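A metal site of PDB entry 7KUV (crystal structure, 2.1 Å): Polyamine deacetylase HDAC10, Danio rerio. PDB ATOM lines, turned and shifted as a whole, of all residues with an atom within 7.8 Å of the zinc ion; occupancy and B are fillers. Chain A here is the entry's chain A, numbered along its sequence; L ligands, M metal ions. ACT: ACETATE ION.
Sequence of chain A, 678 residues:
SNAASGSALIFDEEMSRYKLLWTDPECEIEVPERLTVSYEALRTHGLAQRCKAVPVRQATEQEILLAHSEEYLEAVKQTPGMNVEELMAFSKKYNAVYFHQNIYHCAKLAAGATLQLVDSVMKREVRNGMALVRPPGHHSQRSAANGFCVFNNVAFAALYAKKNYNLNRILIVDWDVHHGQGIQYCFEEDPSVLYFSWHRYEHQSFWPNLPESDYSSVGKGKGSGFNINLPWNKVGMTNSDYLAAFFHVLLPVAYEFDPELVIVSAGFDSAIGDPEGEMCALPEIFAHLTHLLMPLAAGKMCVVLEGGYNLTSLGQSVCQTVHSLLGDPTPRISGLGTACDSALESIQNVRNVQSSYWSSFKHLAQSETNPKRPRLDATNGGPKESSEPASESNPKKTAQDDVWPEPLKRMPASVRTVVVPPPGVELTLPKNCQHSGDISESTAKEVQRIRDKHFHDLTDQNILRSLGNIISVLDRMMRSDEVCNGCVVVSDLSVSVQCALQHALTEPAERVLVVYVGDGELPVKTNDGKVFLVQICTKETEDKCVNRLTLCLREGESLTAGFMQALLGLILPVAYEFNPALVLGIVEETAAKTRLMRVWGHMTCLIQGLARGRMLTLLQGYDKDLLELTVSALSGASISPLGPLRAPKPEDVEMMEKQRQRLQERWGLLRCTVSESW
The side-chain carboxylate of Asp 176 lies within hydrogen-bond range of the backbone NH of Gly 307 (2.9 Å). The side-chain carboxylate (OD2) of Asp 174 sits close to the backbone NH (N) of Asp 176 (3.2 Å). N of Val 177 sits at hydrogen-bond distance from OD1 of Asp 269 (2.8 Å). NE2 of His 178 sits at hydrogen-bond distance from OE1 of Glu 276, at 3.5 Å.
The zinc ion is bound by OD2 of Asp 176, OD2 of Asp 269, ND1 of His 178, O of the ligand and OXT of the ligand. Slightly farther from the zinc ion lies the side-chain carboxylate (OD1) of Asp 176 (2.7 Å).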
ATOM      1  N   PRO A 136     -17.544  -0.202  -3.801  1.00  0.00           N
ATOM      2  CA  PRO A 136     -18.830  -0.883  -3.999  1.00  0.00           C
ATOM      3  C   PRO A 136     -18.696  -2.000  -5.030  1.00  0.00           C
ATOM      4  O   PRO A 136     -17.664  -2.187  -5.679  1.00  0.00           O
ATOM      5  CB  PRO A 136     -19.762   0.229  -4.482  1.00  0.00           C
ATOM      6  CG  PRO A 136     -18.827   1.239  -5.149  1.00  0.00           C
ATOM      7  CD  PRO A 136     -17.565   1.187  -4.325  1.00  0.00           C
ATOM      8  N   HIS A 138     -21.916  -3.624  -6.958  1.00  0.00           N
ATOM      9  CA  HIS A 138     -23.047  -4.192  -7.709  1.00  0.00           C
ATOM     10  C   HIS A 138     -22.966  -3.937  -9.217  1.00  0.00           C
ATOM     11  O   HIS A 138     -23.624  -4.652  -9.983  1.00  0.00           O
ATOM     12  CB  HIS A 138     -24.401  -3.731  -7.123  1.00  0.00           C
ATOM     13  CG  HIS A 138     -24.770  -2.300  -7.390  1.00  0.00           C
ATOM     14  ND1 HIS A 138     -26.088  -1.865  -7.383  1.00  0.00           N
ATOM     15  CD2 HIS A 138     -24.014  -1.210  -7.619  1.00  0.00           C
ATOM     16  CE1 HIS A 138     -26.118  -0.566  -7.612  1.00  0.00           C
ATOM     17  NE2 HIS A 138     -24.869  -0.145  -7.755  1.00  0.00           N
ATOM     18  N   HIS A 139     -22.152  -2.987  -9.686  1.00  0.00           N
ATOM     19  CA  HIS A 139     -21.957  -2.857 -11.132  1.00  0.00           C
ATOM     20  C   HIS A 139     -20.896  -3.802 -11.658  1.00  0.00           C
ATOM     21  O   HIS A 139     -20.805  -3.989 -12.888  1.00  0.00           O
ATOM     22  CB  HIS A 139     -21.541  -1.442 -11.507  1.00  0.00           C
ATOM     23  CG  HIS A 139     -22.544  -0.404 -11.133  1.00  0.00           C
ATOM     24  ND1 HIS A 139     -23.889  -0.516 -11.437  1.00  0.00           N
ATOM     25  CD2 HIS A 139     -22.409   0.770 -10.467  1.00  0.00           C
ATOM     26  CE1 HIS A 139     -24.525   0.542 -10.979  1.00  0.00           C
ATOM     27  NE2 HIS A 139     -23.659   1.336 -10.383  1.00  0.00           N
ATOM     28  N   GLY A 147     -18.490   1.365 -12.979  1.00  0.00           N
ATOM     29  CA  GLY A 147     -19.201   2.239 -12.063  1.00  0.00           C
ATOM     30  C   GLY A 147     -18.698   2.193 -10.617  1.00  0.00           C
ATOM     31  O   GLY A 147     -19.467   1.894  -9.700  1.00  0.00           O
ATOM     32  N   PHE A 148     -17.400   2.463 -10.426  1.00  0.00           N
ATOM     33  CA  PHE A 148     -16.698   2.489  -9.132  1.00  0.00           C
ATOM     34  C   PHE A 148     -16.519   1.107  -8.532  1.00  0.00           C
ATOM     35  O   PHE A 148     -15.897   1.001  -7.477  1.00  0.00           O
ATOM     36  CB  PHE A 148     -17.394   3.376  -8.084  1.00  0.00           C
ATOM     37  CG  PHE A 148     -17.842   4.732  -8.604  1.00  0.00           C
ATOM     38  CD1 PHE A 148     -17.118   5.406  -9.560  1.00  0.00           C
ATOM     39  CD2 PHE A 148     -18.989   5.337  -8.082  1.00  0.00           C
ATOM     40  CE1 PHE A 148     -17.538   6.642 -10.036  1.00  0.00           C
ATOM     41  CE2 PHE A 148     -19.399   6.585  -8.543  1.00  0.00           C
ATOM     42  CZ  PHE A 148     -18.682   7.233  -9.512  1.00  0.00           C
ATOM     43  N   ASP A 174     -31.704  -4.449  -4.025  1.00  0.00           N
ATOM     44  CA  ASP A 174     -30.772  -3.393  -4.430  1.00  0.00           C
ATOM     45  C   ASP A 174     -31.546  -2.071  -4.462  1.00  0.00           C
ATOM     46  O   ASP A 174     -32.174  -1.723  -5.463  1.00  0.00           O
ATOM     47  CB  ASP A 174     -30.133  -3.712  -5.771  1.00  0.00           C
ATOM     48  CG  ASP A 174     -29.032  -2.739  -6.146  1.00  0.00           C
ATOM     49  OD1 ASP A 174     -28.214  -3.149  -7.001  1.00  0.00           O
ATOM     50  OD2 ASP A 174     -28.960  -1.600  -5.617  1.00  0.00           O
ATOM     51  N   TRP A 175     -31.459  -1.328  -3.364  1.00  0.00           N
ATOM     52  CA  TRP A 175     -32.145  -0.046  -3.255  1.00  0.00           C
ATOM     53  C   TRP A 175     -31.220   1.127  -3.530  1.00  0.00           C
ATOM     54  O   TRP A 175     -31.648   2.280  -3.415  1.00  0.00           O
ATOM     55  CB  TRP A 175     -32.852   0.051  -1.896  1.00  0.00           C
ATOM     56  CG  TRP A 175     -32.018   0.291  -0.641  1.00  0.00           C
ATOM     57  CD1 TRP A 175     -30.954   1.158  -0.484  1.00  0.00           C
ATOM     58  CD2 TRP A 175     -32.259  -0.284   0.649  1.00  0.00           C
ATOM     59  NE1 TRP A 175     -30.509   1.124   0.830  1.00  0.00           N
ATOM     60  CE2 TRP A 175     -31.291   0.241   1.533  1.00  0.00           C
ATOM     61  CE3 TRP A 175     -33.190  -1.211   1.141  1.00  0.00           C
ATOM     62  CZ2 TRP A 175     -31.248  -0.109   2.889  1.00  0.00           C
ATOM     63  CZ3 TRP A 175     -33.135  -1.568   2.480  1.00  0.00           C
ATOM     64  CH2 TRP A 175     -32.184  -1.021   3.338  1.00  0.00           C
ATOM     65  N   ASP A 176     -29.976   0.861  -3.919  1.00  0.00           N
ATOM     66  CA  ASP A 176     -29.143   1.871  -4.539  1.00  0.00           C
ATOM     67  C   ASP A 176     -29.910   2.501  -5.694  1.00  0.00           C
ATOM     68  O   ASP A 176     -30.804   1.871  -6.276  1.00  0.00           O
ATOM     69  CB  ASP A 176     -27.828   1.229  -5.014  1.00  0.00           C
ATOM     70  CG  ASP A 176     -26.809   2.237  -5.517  1.00  0.00           C
ATOM     71  OD1 ASP A 176     -25.848   2.537  -4.776  1.00  0.00           O
ATOM     72  OD2 ASP A 176     -26.959   2.734  -6.653  1.00  0.00           O
ATOM     73  N   VAL A 177     -29.594   3.763  -6.017  1.00  0.00           N
ATOM     74  CA  VAL A 177     -30.319   4.484  -7.071  1.00  0.00           C
ATOM     75  C   VAL A 177     -29.892   4.064  -8.466  1.00  0.00           C
ATOM     76  O   VAL A 177     -30.560   4.425  -9.449  1.00  0.00           O
ATOM     77  CB  VAL A 177     -30.151   6.010  -6.908  1.00  0.00           C
ATOM     78  CG1 VAL A 177     -28.871   6.492  -7.587  1.00  0.00           C
ATOM     79  CG2 VAL A 177     -31.385   6.752  -7.464  1.00  0.00           C
ATOM     80  N   HIS A 178     -28.797   3.311  -8.589  1.00  0.00           N
ATOM     81  CA  HIS A 178     -28.317   2.810  -9.864  1.00  0.00           C
ATOM     82  C   HIS A 178     -28.702   1.344 -10.022  1.00  0.00           C
ATOM     83  O   HIS A 178     -28.856   0.607  -9.030  1.00  0.00           O
ATOM     84  CB  HIS A 178     -26.792   2.948  -9.979  1.00  0.00           C
ATOM     85  CG  HIS A 178     -26.306   4.368  -9.985  1.00  0.00           C
ATOM     86  ND1 HIS A 178     -25.898   5.019  -8.843  1.00  0.00           N
ATOM     87  CD2 HIS A 178     -26.150   5.250 -11.004  1.00  0.00           C
ATOM     88  CE1 HIS A 178     -25.503   6.244  -9.154  1.00  0.00           C
ATOM     89  NE2 HIS A 178     -25.647   6.412 -10.460  1.00  0.00           N
ATOM     90  N   HIS A 179     -28.841   0.907 -11.271  1.00  0.00           N
ATOM     91  CA  HIS A 179     -29.144  -0.489 -11.526  1.00  0.00           C
ATOM     92  C   HIS A 179     -27.925  -1.362 -11.278  1.00  0.00           C
ATOM     93  O   HIS A 179     -26.843  -1.108 -11.818  1.00  0.00           O
ATOM     94  CB  HIS A 179     -29.617  -0.678 -12.969  1.00  0.00           C
ATOM     95  CG  HIS A 179     -29.972  -2.097 -13.288  1.00  0.00           C
ATOM     96  ND1 HIS A 179     -29.595  -2.717 -14.463  1.00  0.00           N
ATOM     97  CD2 HIS A 179     -30.693  -3.024 -12.599  1.00  0.00           C
ATOM     98  CE1 HIS A 179     -30.059  -3.951 -14.479  1.00  0.00           C
ATOM     99  NE2 HIS A 179     -30.738  -4.156 -13.359  1.00  0.00           N
ATOM    100  N   PHE A 206     -30.439   7.442 -18.302  1.00  0.00           N
ATOM    101  CA  PHE A 206     -29.578   7.576 -17.133  1.00  0.00           C
ATOM    102  C   PHE A 206     -28.626   6.385 -17.027  1.00  0.00           C
ATOM    103  O   PHE A 206     -29.007   5.241 -17.277  1.00  0.00           O
ATOM    104  CB  PHE A 206     -30.388   7.733 -15.840  1.00  0.00           C
ATOM    105  CG  PHE A 206     -29.533   8.083 -14.643  1.00  0.00           C
ATOM    106  CD1 PHE A 206     -28.924   9.328 -14.550  1.00  0.00           C
ATOM    107  CD2 PHE A 206     -29.307   7.149 -13.625  1.00  0.00           C
ATOM    108  CE1 PHE A 206     -28.107   9.654 -13.459  1.00  0.00           C
ATOM    109  CE2 PHE A 206     -28.498   7.475 -12.521  1.00  0.00           C
ATOM    110  CZ  PHE A 206     -27.897   8.721 -12.457  1.00  0.00           C
ATOM    111  N   TRP A 207     -27.382   6.685 -16.661  1.00  0.00           N
ATOM    112  CA  TRP A 207     -26.343   5.678 -16.563  1.00  0.00           C
ATOM    113  C   TRP A 207     -26.826   4.505 -15.703  1.00  0.00           C
ATOM    114  O   TRP A 207     -27.458   4.722 -14.664  1.00  0.00           O
ATOM    115  CB  TRP A 207     -25.075   6.309 -15.959  1.00  0.00           C
ATOM    116  CG  TRP A 207     -23.879   5.415 -16.069  1.00  0.00           C
ATOM    117  CD1 TRP A 207     -22.927   5.425 -17.045  1.00  0.00           C
ATOM    118  CD2 TRP A 207     -23.537   4.357 -15.175  1.00  0.00           C
ATOM    119  NE1 TRP A 207     -22.000   4.426 -16.824  1.00  0.00           N
ATOM    120  CE2 TRP A 207     -22.359   3.755 -15.688  1.00  0.00           C
ATOM    121  CE3 TRP A 207     -24.110   3.839 -14.012  1.00  0.00           C
ATOM    122  CZ2 TRP A 207     -21.731   2.668 -15.054  1.00  0.00           C
ATOM    123  CZ3 TRP A 207     -23.496   2.755 -13.378  1.00  0.00           C
ATOM    124  CH2 TRP A 207     -22.327   2.178 -13.911  1.00  0.00           C
ATOM    125  N   ALA A 266     -27.096  -1.938  -0.515  1.00  0.00           N
ATOM    126  CA  ALA A 266     -27.654  -0.779   0.164  1.00  0.00           C
ATOM    127  C   ALA A 266     -26.897   0.469  -0.280  1.00  0.00           C
ATOM    128  O   ALA A 266     -25.930   0.906   0.371  1.00  0.00           O
ATOM    129  CB  ALA A 266     -27.592  -0.942   1.685  1.00  0.00           C
ATOM    130  N   GLY A 267     -27.344   1.059  -1.381  1.00  0.00           N
ATOM    131  CA  GLY A 267     -26.872   2.365  -1.808  1.00  0.00           C
ATOM    132  C   GLY A 267     -27.812   3.430  -1.290  1.00  0.00           C
ATOM    133  O   GLY A 267     -29.030   3.308  -1.414  1.00  0.00           O
ATOM    134  N   PHE A 268     -27.241   4.461  -0.703  1.00  0.00           N
ATOM    135  CA  PHE A 268     -28.041   5.551  -0.168  1.00  0.00           C
ATOM    136  C   PHE A 268     -28.001   6.775  -1.087  1.00  0.00           C
ATOM    137  O   PHE A 268     -28.479   7.853  -0.700  1.00  0.00           O
ATOM    138  CB  PHE A 268     -27.599   5.872   1.271  1.00  0.00           C
ATOM    139  CG  PHE A 268     -27.734   4.676   2.210  1.00  0.00           C
ATOM    140  CD1 PHE A 268     -28.994   4.266   2.649  1.00  0.00           C
ATOM    141  CD2 PHE A 268     -26.615   3.934   2.592  1.00  0.00           C
ATOM    142  CE1 PHE A 268     -29.146   3.154   3.466  1.00  0.00           C
ATOM    143  CE2 PHE A 268     -26.755   2.807   3.439  1.00  0.00           C
ATOM    144  CZ  PHE A 268     -28.023   2.424   3.876  1.00  0.00           C
ATOM    145  N   ASP A 269     -27.467   6.620  -2.304  1.00  0.00           N
ATOM    146  CA  ASP A 269     -27.689   7.646  -3.301  1.00  0.00           C
ATOM    147  C   ASP A 269     -29.145   7.705  -3.762  1.00  0.00           C
ATOM    148  O   ASP A 269     -29.452   8.540  -4.626  1.00  0.00           O
ATOM    149  CB  ASP A 269     -26.755   7.481  -4.514  1.00  0.00           C
ATOM    150  CG  ASP A 269     -26.718   6.070  -5.087  1.00  0.00           C
ATOM    151  OD1 ASP A 269     -27.570   5.207  -4.726  1.00  0.00           O
ATOM    152  OD2 ASP A 269     -25.828   5.841  -5.943  1.00  0.00           O
ATOM    153  N   SER A 270     -30.028   6.871  -3.223  1.00  0.00           N
ATOM    154  CA  SER A 270     -31.469   7.010  -3.428  1.00  0.00           C
ATOM    155  C   SER A 270     -32.117   7.972  -2.423  1.00  0.00           C
ATOM    156  O   SER A 270     -33.342   8.134  -2.435  1.00  0.00           O
ATOM    157  CB  SER A 270     -32.122   5.639  -3.312  1.00  0.00           C
ATOM    158  OG  SER A 270     -31.629   4.996  -2.137  1.00  0.00           O
ATOM    159  N   ASP A 274     -28.782  13.603  -2.615  1.00  0.00           N
ATOM    160  CA  ASP A 274     -27.707  12.968  -3.344  1.00  0.00           C
ATOM    161  C   ASP A 274     -27.546  13.584  -4.728  1.00  0.00           C
ATOM    162  O   ASP A 274     -28.536  13.736  -5.455  1.00  0.00           O
ATOM    163  CB  ASP A 274     -27.954  11.470  -3.471  1.00  0.00           C
ATOM    164  CG  ASP A 274     -26.743  10.750  -3.992  1.00  0.00           C
ATOM    165  OD1 ASP A 274     -26.568  10.680  -5.227  1.00  0.00           O
ATOM    166  OD2 ASP A 274     -25.945  10.288  -3.149  1.00  0.00           O
ATOM    167  N   GLU A 276     -26.252  12.316  -7.462  1.00  0.00           N
ATOM    168  CA  GLU A 276     -26.472  11.329  -8.522  1.00  0.00           C
ATOM    169  C   GLU A 276     -27.919  10.880  -8.643  1.00  0.00           C
ATOM    170  O   GLU A 276     -28.425  10.722  -9.762  1.00  0.00           O
ATOM    171  CB  GLU A 276     -25.602  10.094  -8.293  1.00  0.00           C
ATOM    172  CG  GLU A 276     -24.140  10.290  -8.581  1.00  0.00           C
ATOM    173  CD  GLU A 276     -23.864  10.453 -10.060  1.00  0.00           C
ATOM    174  OE1 GLU A 276     -24.298   9.593 -10.873  1.00  0.00           O
ATOM    175  OE2 GLU A 276     -23.219  11.468 -10.405  1.00  0.00           O
ATOM    176  N   GLY A 277     -28.566  10.602  -7.515  1.00  0.00           N
ATOM    177  CA  GLY A 277     -29.927  10.090  -7.562  1.00  0.00           C
ATOM    178  C   GLY A 277     -30.948  11.179  -7.860  1.00  0.00           C
ATOM    179  O   GLY A 277     -31.868  10.981  -8.648  1.00  0.00           O
ATOM    180  N   GLU A 306     -23.289   0.093  -0.851  1.00  0.00           N
ATOM    181  CA  GLU A 306     -22.948   0.350  -2.248  1.00  0.00           C
ATOM    182  C   GLU A 306     -22.619   1.827  -2.410  1.00  0.00           C
ATOM    183  O   GLU A 306     -21.516   2.249  -2.000  1.00  0.00           O
ATOM    184  CB  GLU A 306     -24.090  -0.138  -3.167  1.00  0.00           C
ATOM    185  CG  GLU A 306     -24.378  -1.626  -3.006  1.00  0.00           C
ATOM    186  CD  GLU A 306     -23.511  -2.519  -3.930  1.00  0.00           C
ATOM    187  OE1 GLU A 306     -22.658  -1.983  -4.676  1.00  0.00           O
ATOM    188  OE2 GLU A 306     -23.704  -3.751  -3.935  1.00  0.00           O
ATOM    189  N   GLY A 307     -23.483   2.640  -3.018  1.00  0.00           N
ATOM    190  CA  GLY A 307     -23.218   4.051  -3.219  1.00  0.00           C
ATOM    191  C   GLY A 307     -23.842   4.931  -2.146  1.00  0.00           C
ATOM    192  O   GLY A 307     -24.348   4.458  -1.122  1.00  0.00           O
ATOM    193  N   GLY A 308     -23.816   6.249  -2.399  1.00  0.00           N
ATOM    194  CA  GLY A 308     -24.332   7.271  -1.488  1.00  0.00           C
ATOM    195  C   GLY A 308     -23.326   8.403  -1.324  1.00  0.00           C
ATOM    196  O   GLY A 308     -22.252   8.196  -0.746  1.00  0.00           O
ATOM    197  N   TYR A 309     -23.628   9.598  -1.854  1.00  0.00           N
ATOM    198  CA  TYR A 309     -22.565  10.557  -2.137  1.00  0.00           C
ATOM    199  C   TYR A 309     -22.708  11.919  -1.497  1.00  0.00           C
ATOM    200  O   TYR A 309     -21.773  12.712  -1.590  1.00  0.00           O
ATOM    201  CB  TYR A 309     -22.402  10.736  -3.658  1.00  0.00           C
ATOM    202  CG  TYR A 309     -22.117   9.411  -4.312  1.00  0.00           C
ATOM    203  CD1 TYR A 309     -20.853   8.854  -4.240  1.00  0.00           C
ATOM    204  CD2 TYR A 309     -23.127   8.680  -4.924  1.00  0.00           C
ATOM    205  CE1 TYR A 309     -20.574   7.628  -4.797  1.00  0.00           C
ATOM    206  CE2 TYR A 309     -22.873   7.445  -5.496  1.00  0.00           C
ATOM    207  CZ  TYR A 309     -21.598   6.927  -5.425  1.00  0.00           C
ATOM    208  OH  TYR A 309     -21.328   5.698  -5.986  1.00  0.00           O
HETATM  209  C   ACT L   1     -23.158   3.065  -7.244  1.00  0.00           C
HETATM  210  O   ACT L   1     -23.304   4.291  -6.970  1.00  0.00           O
HETATM  211  OXT ACT L   1     -24.032   2.216  -7.609  1.00  0.00           O
HETATM  212  CH3 ACT L   1     -21.716   2.504  -7.102  1.00  0.00           C
HETATM  213 ZN    ZN M   1     -25.545   4.090  -6.939  1.00  0.00          ZN
